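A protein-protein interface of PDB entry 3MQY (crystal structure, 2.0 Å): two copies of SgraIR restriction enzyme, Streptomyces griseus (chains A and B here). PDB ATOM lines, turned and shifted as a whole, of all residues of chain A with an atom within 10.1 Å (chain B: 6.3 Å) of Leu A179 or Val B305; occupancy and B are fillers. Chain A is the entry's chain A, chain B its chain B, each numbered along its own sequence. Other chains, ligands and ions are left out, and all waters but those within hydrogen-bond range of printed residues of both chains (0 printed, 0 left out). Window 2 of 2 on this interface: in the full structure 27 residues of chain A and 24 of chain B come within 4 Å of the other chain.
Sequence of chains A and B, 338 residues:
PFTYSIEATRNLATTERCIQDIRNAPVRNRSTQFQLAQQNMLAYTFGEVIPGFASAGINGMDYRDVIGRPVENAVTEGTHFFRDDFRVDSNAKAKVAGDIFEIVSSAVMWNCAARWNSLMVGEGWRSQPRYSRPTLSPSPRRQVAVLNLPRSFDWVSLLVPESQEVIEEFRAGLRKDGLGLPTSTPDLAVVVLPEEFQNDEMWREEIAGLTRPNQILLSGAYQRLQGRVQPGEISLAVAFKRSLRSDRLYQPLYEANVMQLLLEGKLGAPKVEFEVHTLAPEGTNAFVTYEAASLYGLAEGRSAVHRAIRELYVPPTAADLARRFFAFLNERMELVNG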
ATOM      1  N   ILE A 167       7.503  -3.425 -35.614  1.00  0.00           N
ATOM      2  CA  ILE A 167       7.276  -2.273 -34.720  1.00  0.00           C
ATOM      3  C   ILE A 167       5.807  -1.991 -34.613  1.00  0.00           C
ATOM      4  O   ILE A 167       5.324  -1.696 -33.544  1.00  0.00           O
ATOM      5  CB  ILE A 167       8.065  -0.983 -35.182  1.00  0.00           C
ATOM      6  CG1 ILE A 167       9.546  -1.187 -34.930  1.00  0.00           C
ATOM      7  CG2 ILE A 167       7.608   0.285 -34.445  1.00  0.00           C
ATOM      8  CD1 ILE A 167      10.437  -0.256 -35.718  1.00  0.00           C
ATOM      9  N   GLU A 168       5.087  -2.097 -35.715  1.00  0.00           N
ATOM     10  CA  GLU A 168       3.674  -1.738 -35.718  1.00  0.00           C
ATOM     11  C   GLU A 168       2.783  -2.793 -35.001  1.00  0.00           C
ATOM     12  O   GLU A 168       1.806  -2.445 -34.349  1.00  0.00           O
ATOM     13  CB  GLU A 168       3.214  -1.444 -37.141  1.00  0.00           C
ATOM     14  CG  GLU A 168       1.725  -1.332 -37.338  1.00  0.00           C
ATOM     15  CD  GLU A 168       1.084  -0.382 -36.369  1.00  0.00           C
ATOM     16  OE1 GLU A 168      -0.152  -0.462 -36.156  1.00  0.00           O
ATOM     17  OE2 GLU A 168       1.826   0.449 -35.810  1.00  0.00           O
ATOM     18  N   GLU A 169       3.128  -4.069 -35.082  1.00  0.00           N
ATOM     19  CA  GLU A 169       2.385  -5.069 -34.293  1.00  0.00           C
ATOM     20  C   GLU A 169       2.574  -4.884 -32.772  1.00  0.00           C
ATOM     21  O   GLU A 169       1.618  -4.955 -31.991  1.00  0.00           O
ATOM     22  CB  GLU A 169       2.771  -6.493 -34.717  1.00  0.00           C
ATOM     23  CG  GLU A 169       1.835  -7.068 -35.771  1.00  0.00           C
ATOM     24  CD  GLU A 169       0.561  -7.678 -35.162  1.00  0.00           C
ATOM     25  OE1 GLU A 169      -0.549  -7.080 -35.342  1.00  0.00           O
ATOM     26  OE2 GLU A 169       0.686  -8.746 -34.495  1.00  0.00           O
ATOM     27  N   PHE A 170       3.817  -4.646 -32.372  1.00  0.00           N
ATOM     28  CA  PHE A 170       4.144  -4.298 -31.008  1.00  0.00           C
ATOM     29  C   PHE A 170       3.376  -3.053 -30.528  1.00  0.00           C
ATOM     30  O   PHE A 170       2.849  -3.052 -29.423  1.00  0.00           O
ATOM     31  CB  PHE A 170       5.669  -4.120 -30.887  1.00  0.00           C
ATOM     32  CG  PHE A 170       6.127  -3.627 -29.520  1.00  0.00           C
ATOM     33  CD1 PHE A 170       5.962  -4.422 -28.386  1.00  0.00           C
ATOM     34  CD2 PHE A 170       6.689  -2.359 -29.372  1.00  0.00           C
ATOM     35  CE1 PHE A 170       6.359  -3.983 -27.125  1.00  0.00           C
ATOM     36  CE2 PHE A 170       7.102  -1.920 -28.119  1.00  0.00           C
ATOM     37  CZ  PHE A 170       6.934  -2.748 -26.983  1.00  0.00           C
ATOM     38  N   ARG A 171       3.297  -2.003 -31.351  1.00  0.00           N
ATOM     39  CA  ARG A 171       2.500  -0.808 -30.980  1.00  0.00           C
ATOM     40  C   ARG A 171       1.005  -1.055 -30.946  1.00  0.00           C
ATOM     41  O   ARG A 171       0.300  -0.467 -30.115  1.00  0.00           O
ATOM     42  CB  ARG A 171       2.732   0.333 -31.958  1.00  0.00           C
ATOM     43  CG  ARG A 171       4.015   1.068 -31.746  1.00  0.00           C
ATOM     44  CD  ARG A 171       4.151   2.114 -32.811  1.00  0.00           C
ATOM     45  NE  ARG A 171       5.323   2.957 -32.581  1.00  0.00           N
ATOM     46  CZ  ARG A 171       5.990   3.575 -33.545  1.00  0.00           C
ATOM     47  NH1 ARG A 171       5.673   3.389 -34.803  1.00  0.00           N
ATOM     48  NH2 ARG A 171       7.023   4.319 -33.233  1.00  0.00           N
ATOM     49  N   ALA A 172       0.517  -1.873 -31.880  1.00  0.00           N
ATOM     50  CA  ALA A 172      -0.885  -2.281 -31.885  1.00  0.00           C
ATOM     51  C   ALA A 172      -1.271  -2.937 -30.561  1.00  0.00           C
ATOM     52  O   ALA A 172      -2.319  -2.606 -29.987  1.00  0.00           O
ATOM     53  CB  ALA A 172      -1.178  -3.230 -33.048  1.00  0.00           C
ATOM     54  N   GLY A 173      -0.432  -3.853 -30.074  1.00  0.00           N
ATOM     55  CA  GLY A 173      -0.603  -4.423 -28.726  1.00  0.00           C
ATOM     56  C   GLY A 173      -0.636  -3.349 -27.628  1.00  0.00           C
ATOM     57  O   GLY A 173      -1.545  -3.314 -26.788  1.00  0.00           O
ATOM     58  N   LEU A 174       0.337  -2.441 -27.643  1.00  0.00           N
ATOM     59  CA  LEU A 174       0.352  -1.358 -26.675  1.00  0.00           C
ATOM     60  C   LEU A 174      -0.923  -0.495 -26.718  1.00  0.00           C
ATOM     61  O   LEU A 174      -1.394  -0.073 -25.690  1.00  0.00           O
ATOM     62  CB  LEU A 174       1.590  -0.474 -26.850  1.00  0.00           C
ATOM     63  CG  LEU A 174       2.955  -1.107 -26.623  1.00  0.00           C
ATOM     64  CD1 LEU A 174       3.973  -0.004 -26.431  1.00  0.00           C
ATOM     65  CD2 LEU A 174       2.993  -2.104 -25.445  1.00  0.00           C
ATOM     66  N   ARG A 175      -1.473  -0.221 -27.886  1.00  0.00           N
ATOM     67  CA  ARG A 175      -2.732   0.549 -27.930  1.00  0.00           C
ATOM     68  C   ARG A 175      -3.906  -0.089 -27.191  1.00  0.00           C
ATOM     69  O   ARG A 175      -4.694   0.621 -26.597  1.00  0.00           O
ATOM     70  CB  ARG A 175      -3.154   0.867 -29.361  1.00  0.00           C
ATOM     71  CG  ARG A 175      -2.774   2.303 -29.779  1.00  0.00           C
ATOM     72  CD  ARG A 175      -3.089   2.573 -31.260  1.00  0.00           C
ATOM     73  NE  ARG A 175      -2.570   1.528 -32.164  1.00  0.00           N
ATOM     74  CZ  ARG A 175      -1.432   1.591 -32.864  1.00  0.00           C
ATOM     75  NH1 ARG A 175      -0.643   2.655 -32.801  1.00  0.00           N
ATOM     76  NH2 ARG A 175      -1.072   0.564 -33.635  1.00  0.00           N
ATOM     77  N   LYS A 176      -4.028  -1.417 -27.232  1.00  0.00           N
ATOM     78  CA  LYS A 176      -5.128  -2.108 -26.518  1.00  0.00           C
ATOM     79  C   LYS A 176      -5.140  -1.628 -25.084  1.00  0.00           C
ATOM     80  O   LYS A 176      -6.189  -1.265 -24.554  1.00  0.00           O
ATOM     81  CB  LYS A 176      -4.992  -3.644 -26.560  1.00  0.00           C
ATOM     82  CG  LYS A 176      -5.287  -4.302 -27.949  1.00  0.00           C
ATOM     83  CD  LYS A 176      -5.923  -5.720 -27.786  1.00  0.00           C
ATOM     84  CE  LYS A 176      -6.275  -6.385 -29.134  1.00  0.00           C
ATOM     85  NZ  LYS A 176      -5.154  -7.246 -29.585  1.00  0.00           N
ATOM     86  N   ASP A 177      -3.953  -1.552 -24.490  1.00  0.00           N
ATOM     87  CA  ASP A 177      -3.788  -1.104 -23.108  1.00  0.00           C
ATOM     88  C   ASP A 177      -3.701   0.424 -22.915  1.00  0.00           C
ATOM     89  O   ASP A 177      -3.295   0.896 -21.847  1.00  0.00           O
ATOM     90  CB  ASP A 177      -2.518  -1.735 -22.530  1.00  0.00           C
ATOM     91  CG  ASP A 177      -2.437  -3.255 -22.757  1.00  0.00           C
ATOM     92  OD1 ASP A 177      -1.432  -3.697 -23.370  1.00  0.00           O
ATOM     93  OD2 ASP A 177      -3.361  -3.988 -22.324  1.00  0.00           O
ATOM     94  N   GLY A 178      -4.074   1.193 -23.934  1.00  0.00           N
ATOM     95  CA  GLY A 178      -3.985   2.664 -23.887  1.00  0.00           C
ATOM     96  C   GLY A 178      -2.567   3.186 -23.652  1.00  0.00           C
ATOM     97  O   GLY A 178      -2.381   4.073 -22.846  1.00  0.00           O
ATOM     98  N   LEU A 179      -1.574   2.603 -24.324  1.00  0.00           N
ATOM     99  CA  LEU A 179      -0.195   3.093 -24.307  1.00  0.00           C
ATOM    100  C   LEU A 179       0.258   3.282 -25.781  1.00  0.00           C
ATOM    101  O   LEU A 179      -0.348   2.743 -26.722  1.00  0.00           O
ATOM    102  CB  LEU A 179       0.755   2.108 -23.571  1.00  0.00           C
ATOM    103  CG  LEU A 179       0.359   1.367 -22.271  1.00  0.00           C
ATOM    104  CD1 LEU A 179       1.063  -0.038 -22.099  1.00  0.00           C
ATOM    105  CD2 LEU A 179       0.556   2.232 -21.031  1.00  0.00           C
ATOM    106  N   GLY A 180       1.350   4.026 -25.975  1.00  0.00           N
ATOM    107  CA  GLY A 180       1.972   4.127 -27.283  1.00  0.00           C
ATOM    108  C   GLY A 180       3.455   4.062 -27.095  1.00  0.00           C
ATOM    109  O   GLY A 180       3.924   4.107 -25.981  1.00  0.00           O
ATOM    110  N   LEU A 181       4.206   3.938 -28.178  1.00  0.00           N
ATOM    111  CA  LEU A 181       5.639   4.263 -28.127  1.00  0.00           C
ATOM    112  C   LEU A 181       6.026   5.045 -29.423  1.00  0.00           C
ATOM    113  O   LEU A 181       6.468   4.477 -30.396  1.00  0.00           O
ATOM    114  CB  LEU A 181       6.510   3.037 -27.909  1.00  0.00           C
ATOM    115  CG  LEU A 181       7.931   3.349 -27.375  1.00  0.00           C
ATOM    116  CD1 LEU A 181       7.912   3.820 -25.930  1.00  0.00           C
ATOM    117  CD2 LEU A 181       8.893   2.178 -27.491  1.00  0.00           C
ATOM    118  N   PRO A 182       5.799   6.362 -29.431  1.00  0.00           N
ATOM    119  CA  PRO A 182       6.209   7.159 -30.567  1.00  0.00           C
ATOM    120  C   PRO A 182       7.720   7.239 -30.812  1.00  0.00           C
ATOM    121  O   PRO A 182       8.508   7.209 -29.897  1.00  0.00           O
ATOM    122  CB  PRO A 182       5.692   8.553 -30.243  1.00  0.00           C
ATOM    123  CG  PRO A 182       4.762   8.412 -29.090  1.00  0.00           C
ATOM    124  CD  PRO A 182       5.081   7.130 -28.411  1.00  0.00           C
ATOM    125  N   LEU A 261      15.859   0.351 -27.495  1.00  0.00           N
ATOM    126  CA  LEU A 261      14.729  -0.540 -27.250  1.00  0.00           C
ATOM    127  C   LEU A 261      14.162  -1.169 -28.521  1.00  0.00           C
ATOM    128  O   LEU A 261      14.013  -2.412 -28.581  1.00  0.00           O
ATOM    129  CB  LEU A 261      13.617   0.142 -26.431  1.00  0.00           C
ATOM    130  CG  LEU A 261      12.371  -0.634 -25.959  1.00  0.00           C
ATOM    131  CD1 LEU A 261      11.543   0.236 -24.997  1.00  0.00           C
ATOM    132  CD2 LEU A 261      11.449  -1.058 -27.010  1.00  0.00           C
ATOM    133  N   LYS A 266      13.824  -5.361 -30.146  1.00  0.00           N
ATOM    134  CA  LYS A 266      12.741  -5.989 -30.923  1.00  0.00           C
ATOM    135  C   LYS A 266      13.163  -6.422 -32.299  1.00  0.00           C
ATOM    136  O   LYS A 266      12.453  -7.127 -32.951  1.00  0.00           O
ATOM    137  CB  LYS A 266      11.534  -5.077 -31.066  1.00  0.00           C
ATOM    138  CG  LYS A 266      10.935  -4.634 -29.758  1.00  0.00           C
ATOM    139  CD  LYS A 266      10.272  -5.801 -28.984  1.00  0.00           C
ATOM    140  CE  LYS A 266       9.619  -5.193 -27.760  1.00  0.00           C
ATOM    141  NZ  LYS A 266       9.222  -6.155 -26.714  1.00  0.00           N
ATOM    142  N   TYR A 296      16.699   0.038 -21.389  1.00  0.00           N
ATOM    143  CA  TYR A 296      16.142  -1.235 -21.752  1.00  0.00           C
ATOM    144  C   TYR A 296      17.016  -2.408 -21.304  1.00  0.00           C
ATOM    145  O   TYR A 296      16.504  -3.422 -20.856  1.00  0.00           O
ATOM    146  CB  TYR A 296      15.925  -1.344 -23.252  1.00  0.00           C
ATOM    147  CG  TYR A 296      14.965  -2.477 -23.627  1.00  0.00           C
ATOM    148  CD1 TYR A 296      13.588  -2.339 -23.419  1.00  0.00           C
ATOM    149  CD2 TYR A 296      15.431  -3.683 -24.196  1.00  0.00           C
ATOM    150  CE1 TYR A 296      12.677  -3.344 -23.778  1.00  0.00           C
ATOM    151  CE2 TYR A 296      14.528  -4.708 -24.554  1.00  0.00           C
ATOM    152  CZ  TYR A 296      13.147  -4.536 -24.325  1.00  0.00           C
ATOM    153  OH  TYR A 296      12.210  -5.509 -24.642  1.00  0.00           O
ATOM    154  N   ARG A 302      17.288  -8.762 -21.219  1.00  0.00           N
ATOM    155  CA  ARG A 302      17.044  -8.016 -22.454  1.00  0.00           C
ATOM    156  C   ARG A 302      18.366  -7.890 -23.294  1.00  0.00           C
ATOM    157  O   ARG A 302      19.200  -8.796 -23.269  1.00  0.00           O
ATOM    158  CB  ARG A 302      16.447  -6.639 -22.112  1.00  0.00           C
ATOM    159  CG  ARG A 302      15.076  -6.688 -21.469  1.00  0.00           C
ATOM    160  CD  ARG A 302      14.077  -7.503 -22.314  1.00  0.00           C
ATOM    161  NE  ARG A 302      12.704  -7.236 -21.902  1.00  0.00           N
ATOM    162  CZ  ARG A 302      11.619  -7.724 -22.491  1.00  0.00           C
ATOM    163  NH1 ARG A 302      11.713  -8.542 -23.532  1.00  0.00           N
ATOM    164  NH2 ARG A 302      10.421  -7.366 -22.025  1.00  0.00           N
ATOM    165  N   GLU B 291       1.730  10.009 -24.270  1.00  0.00           N
ATOM    166  CA  GLU B 291       1.071   8.704 -24.133  1.00  0.00           C
ATOM    167  C   GLU B 291       2.071   7.575 -24.042  1.00  0.00           C
ATOM    168  O   GLU B 291       1.646   6.442 -23.816  1.00  0.00           O
ATOM    169  CB  GLU B 291       0.143   8.437 -25.327  1.00  0.00           C
ATOM    170  CG  GLU B 291      -1.109   9.232 -25.281  1.00  0.00           C
ATOM    171  CD  GLU B 291      -1.916   9.153 -26.574  1.00  0.00           C
ATOM    172  OE1 GLU B 291      -1.480   8.523 -27.586  1.00  0.00           O
ATOM    173  OE2 GLU B 291      -3.019   9.722 -26.546  1.00  0.00           O
ATOM    174  N   ALA B 292       3.380   7.865 -24.214  1.00  0.00           N
ATOM    175  CA  ALA B 292       4.421   6.855 -24.238  1.00  0.00           C
ATOM    176  C   ALA B 292       4.377   5.929 -23.007  1.00  0.00           C
ATOM    177  O   ALA B 292       4.274   6.401 -21.847  1.00  0.00           O
ATOM    178  CB  ALA B 292       5.803   7.493 -24.329  1.00  0.00           C
ATOM    179  N   ALA B 293       4.535   4.624 -23.255  1.00  0.00           N
ATOM    180  CA  ALA B 293       4.784   3.658 -22.150  1.00  0.00           C
ATOM    181  C   ALA B 293       6.114   3.908 -21.456  1.00  0.00           C
ATOM    182  O   ALA B 293       7.125   4.249 -22.080  1.00  0.00           O
ATOM    183  CB  ALA B 293       4.710   2.204 -22.678  1.00  0.00           C
ATOM    184  N   SER B 294       6.139   3.758 -20.140  1.00  0.00           N
ATOM    185  CA  SER B 294       7.404   3.560 -19.422  1.00  0.00           C
ATOM    186  C   SER B 294       8.357   2.587 -20.175  1.00  0.00           C
ATOM    187  O   SER B 294       7.929   1.515 -20.623  1.00  0.00           O
ATOM    188  CB  SER B 294       7.131   2.990 -18.024  1.00  0.00           C
ATOM    189  OG  SER B 294       8.335   2.963 -17.295  1.00  0.00           O
ATOM    190  N   GLY B 297       9.102  -0.103 -17.757  1.00  0.00           N
ATOM    191  CA  GLY B 297       7.878  -0.931 -17.705  1.00  0.00           C
ATOM    192  C   GLY B 297       7.900  -1.934 -18.845  1.00  0.00           C
ATOM    193  O   GLY B 297       7.866  -3.174 -18.623  1.00  0.00           O
ATOM    194  N   LEU B 298       8.056  -1.422 -20.052  1.00  0.00           N
ATOM    195  CA  LEU B 298       8.350  -2.308 -21.185  1.00  0.00           C
ATOM    196  C   LEU B 298       9.572  -3.266 -20.983  1.00  0.00           C
ATOM    197  O   LEU B 298       9.458  -4.418 -21.351  1.00  0.00           O
ATOM    198  CB  LEU B 298       8.502  -1.538 -22.498  1.00  0.00           C
ATOM    199  CG  LEU B 298       7.337  -0.682 -23.007  1.00  0.00           C
ATOM    200  CD1 LEU B 298       7.825   0.181 -24.193  1.00  0.00           C
ATOM    201  CD2 LEU B 298       6.020  -1.435 -23.367  1.00  0.00           C
ATOM    202  N   GLY B 301       8.482  -5.960 -18.488  1.00  0.00           N
ATOM    203  CA  GLY B 301       7.389  -6.676 -19.164  1.00  0.00           C
ATOM    204  C   GLY B 301       6.482  -7.359 -18.153  1.00  0.00           C
ATOM    205  O   GLY B 301       6.149  -8.540 -18.300  1.00  0.00           O
ATOM    206  N   ARG B 302       6.127  -6.612 -17.108  1.00  0.00           N
ATOM    207  CA  ARG B 302       5.289  -7.098 -16.021  1.00  0.00           C
ATOM    208  C   ARG B 302       3.846  -7.109 -16.496  1.00  0.00           C
ATOM    209  O   ARG B 302       3.566  -6.798 -17.652  1.00  0.00           O
ATOM    210  CB  ARG B 302       5.465  -6.231 -14.771  1.00  0.00           C
ATOM    211  CG  ARG B 302       6.913  -6.137 -14.301  1.00  0.00           C
ATOM    212  CD  ARG B 302       7.103  -5.390 -12.986  1.00  0.00           C
ATOM    213  NE  ARG B 302       8.130  -6.056 -12.180  1.00  0.00           N
ATOM    214  CZ  ARG B 302       9.314  -5.558 -11.836  1.00  0.00           C
ATOM    215  NH1 ARG B 302       9.706  -4.329 -12.196  1.00  0.00           N
ATOM    216  NH2 ARG B 302      10.114  -6.319 -11.100  1.00  0.00           N
ATOM    217  N   SER B 303       2.929  -7.474 -15.603  1.00  0.00           N
ATOM    218  CA  SER B 303       1.513  -7.619 -15.958  1.00  0.00           C
ATOM    219  C   SER B 303       0.824  -6.308 -16.396  1.00  0.00           C
ATOM    220  O   SER B 303      -0.055  -6.311 -17.244  1.00  0.00           O
ATOM    221  CB  SER B 303       0.733  -8.200 -14.776  1.00  0.00           C
ATOM    222  OG  SER B 303      -0.661  -8.087 -14.984  1.00  0.00           O
ATOM    223  N   ALA B 304       1.179  -5.205 -15.794  1.00  0.00           N
ATOM    224  CA  ALA B 304       0.586  -3.931 -16.188  1.00  0.00           C
ATOM    225  C   ALA B 304       1.742  -2.971 -16.478  1.00  0.00           C
ATOM    226  O   ALA B 304       2.666  -2.812 -15.686  1.00  0.00           O
ATOM    227  CB  ALA B 304      -0.334  -3.382 -15.060  1.00  0.00           C
ATOM    228  N   VAL B 305       1.718  -2.379 -17.645  1.00  0.00           N
ATOM    229  CA  VAL B 305       2.687  -1.357 -17.970  1.00  0.00           C
ATOM    230  C   VAL B 305       1.882  -0.063 -17.911  1.00  0.00           C
ATOM    231  O   VAL B 305       0.763  -0.001 -18.410  1.00  0.00           O
ATOM    232  CB  VAL B 305       3.280  -1.590 -19.361  1.00  0.00           C
ATOM    233  CG1 VAL B 305       4.253  -0.421 -19.750  1.00  0.00           C
ATOM    234  CG2 VAL B 305       3.997  -2.951 -19.427  1.00  0.00           C
ATOM    235  N   HIS B 306       2.430   0.928 -17.224  1.00  0.00           N
ATOM    236  CA  HIS B 306       1.860   2.263 -17.192  1.00  0.00           C
ATOM    237  C   HIS B 306       2.641   3.259 -18.069  1.00  0.00           C
ATOM    238  O   HIS B 306       3.788   3.030 -18.469  1.00  0.00           O
ATOM    239  CB  HIS B 306       1.843   2.799 -15.767  1.00  0.00           C
ATOM    240  CG  HIS B 306       1.222   1.861 -14.771  1.00  0.00           C
ATOM    241  ND1 HIS B 306       1.976   1.134 -13.873  1.00  0.00           N
ATOM    242  CD2 HIS B 306      -0.078   1.526 -14.541  1.00  0.00           C
ATOM    243  CE1 HIS B 306       1.164   0.402 -13.121  1.00  0.00           C
ATOM    244  NE2 HIS B 306      -0.086   0.623 -13.503  1.00  0.00           N
ATOM    245  N   ARG B 307       2.005   4.396 -18.301  1.00  0.00           N
ATOM    246  CA  ARG B 307       2.659   5.516 -18.950  1.00  0.00           C
ATOM    247  C   ARG B 307       3.720   6.117 -18.076  1.00  0.00           C
ATOM    248  O   ARG B 307       3.570   6.188 -16.858  1.00  0.00           O
ATOM    249  CB  ARG B 307       1.640   6.599 -19.226  1.00  0.00           C
ATOM    250  CG  ARG B 307       0.601   6.183 -20.196  1.00  0.00           C
ATOM    251  CD  ARG B 307      -0.331   7.301 -20.499  1.00  0.00           C
ATOM    252  NE  ARG B 307      -1.204   6.862 -21.568  1.00  0.00           N
ATOM    253  CZ  ARG B 307      -2.241   7.553 -22.026  1.00  0.00           C
ATOM    254  NH1 ARG B 307      -2.538   8.756 -21.506  1.00  0.00           N
ATOM    255  NH2 ARG B 307      -2.974   7.030 -23.004  1.00  0.00           N
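Among the printed residues, pairs that only touch across the chains: Gly A180 with Ala B292 (3.3 Å), Leu A179 with Val B305 (3.4 Å), Leu A174 with Leu B298 (3.7 Å), Leu A179 with His B306 (3.8 Å), Leu A179 with Arg B307 (3.8 Å), Leu A261 with Leu B298 (3.8 Å), Leu A179 with Glu B291 (3.9 Å), Leu A181 with Ala B293 (3.95 Å) and Phe A170 with Leu B298 (3.95 Å).
The guanidinium group (NH2) of Arg B307 sits at hydrogen-bond distance from the backbone carbonyl oxygen (O) of Gly A178 (3.0 Å).
O of Glu B291 is in hydrogen-bond range of N of Gly A180, 3.3 Å away.
The backbone carbonyl oxygen (O) of Gly A180 lies within hydrogen-bond range of the backbone NH (N) of Ala B293 (2.8 Å).
NH2 of Arg A302 is in hydrogen-bond range of O of Leu B298 (3.2 Å).
Leu A179 touches just these residues of chain B: Glu B291, Val B305, His B306 and Arg B307.
Of chain A, only Leu A179 (3.4 Å) comes within 4 Å of Val B305.
No residue of chain A comes within 4 Å of Ser B294.
No residue of chain A comes within 4 Å of Gly B297.
Of the printed residues of chain B, Phe A170 touches Leu B298.
Of the printed residues of chain B, Arg A302 touches Leu B298 (3.2 Å).
Of the printed residues of chain B, Leu A174 touches Leu B298 (3.7 Å).
Of the printed residues of chain B, Leu A181 touches Ala B293 (3.95 Å).
Of the printed residues of chain A, Leu B298 touches Phe A170 (3.95 Å), Leu A174 (3.7 Å), Leu A261 (3.8 Å) and Arg A302 (3.2 Å).
Arg B302 touches none of the printed residues of chain A.
Asp A177 touches none of the printed residues of chain B.
The nearest residue of chain B that does not touch Leu A179 is Ala B293 (4.1 Å).
The nearest printed residue of chain B that does not touch Phe A170 is Ala B293 (6.9 Å).
NH2 of Arg A171 is in hydrogen-bond range of O of Leu A181 (2.9 Å).
The backbone NH (N) of Leu A179 sits at hydrogen-bond distance from the backbone carbonyl oxygen (O) of Leu A174, at 3.0 Å.
The backbone carbonyl oxygen (O) of Leu A261 lies within hydrogen-bond range of the backbone NH (N) of Lys A266 (3.3 Å).
The side-chain hydroxyl (OH) of Tyr A296 sits close to the guanidinium group (NH1) of Arg A302 (3.3 Å).
The backbone NH (N) of Ser B294 sits at hydrogen-bond distance from the backbone carbonyl oxygen (O) of His B306 (3.0 Å).
Of the 20 printed residues of chain A, 8 touch a printed residue of chain B.
Of the 13 printed residues of chain B, 7 touch a printed residue of chain A.
Hydrophobic or aromatic side chains of chain B within 4 Å of the printed part of chain A: Ala B293, Leu B298 and Val B305.
Among the printed residues, 13 pairs touch across the chains.
1 position is printed for both chains.
Of the 13 pairs that touch across the chains among the printed residues, none has its exchanged pair printed and touching as well.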
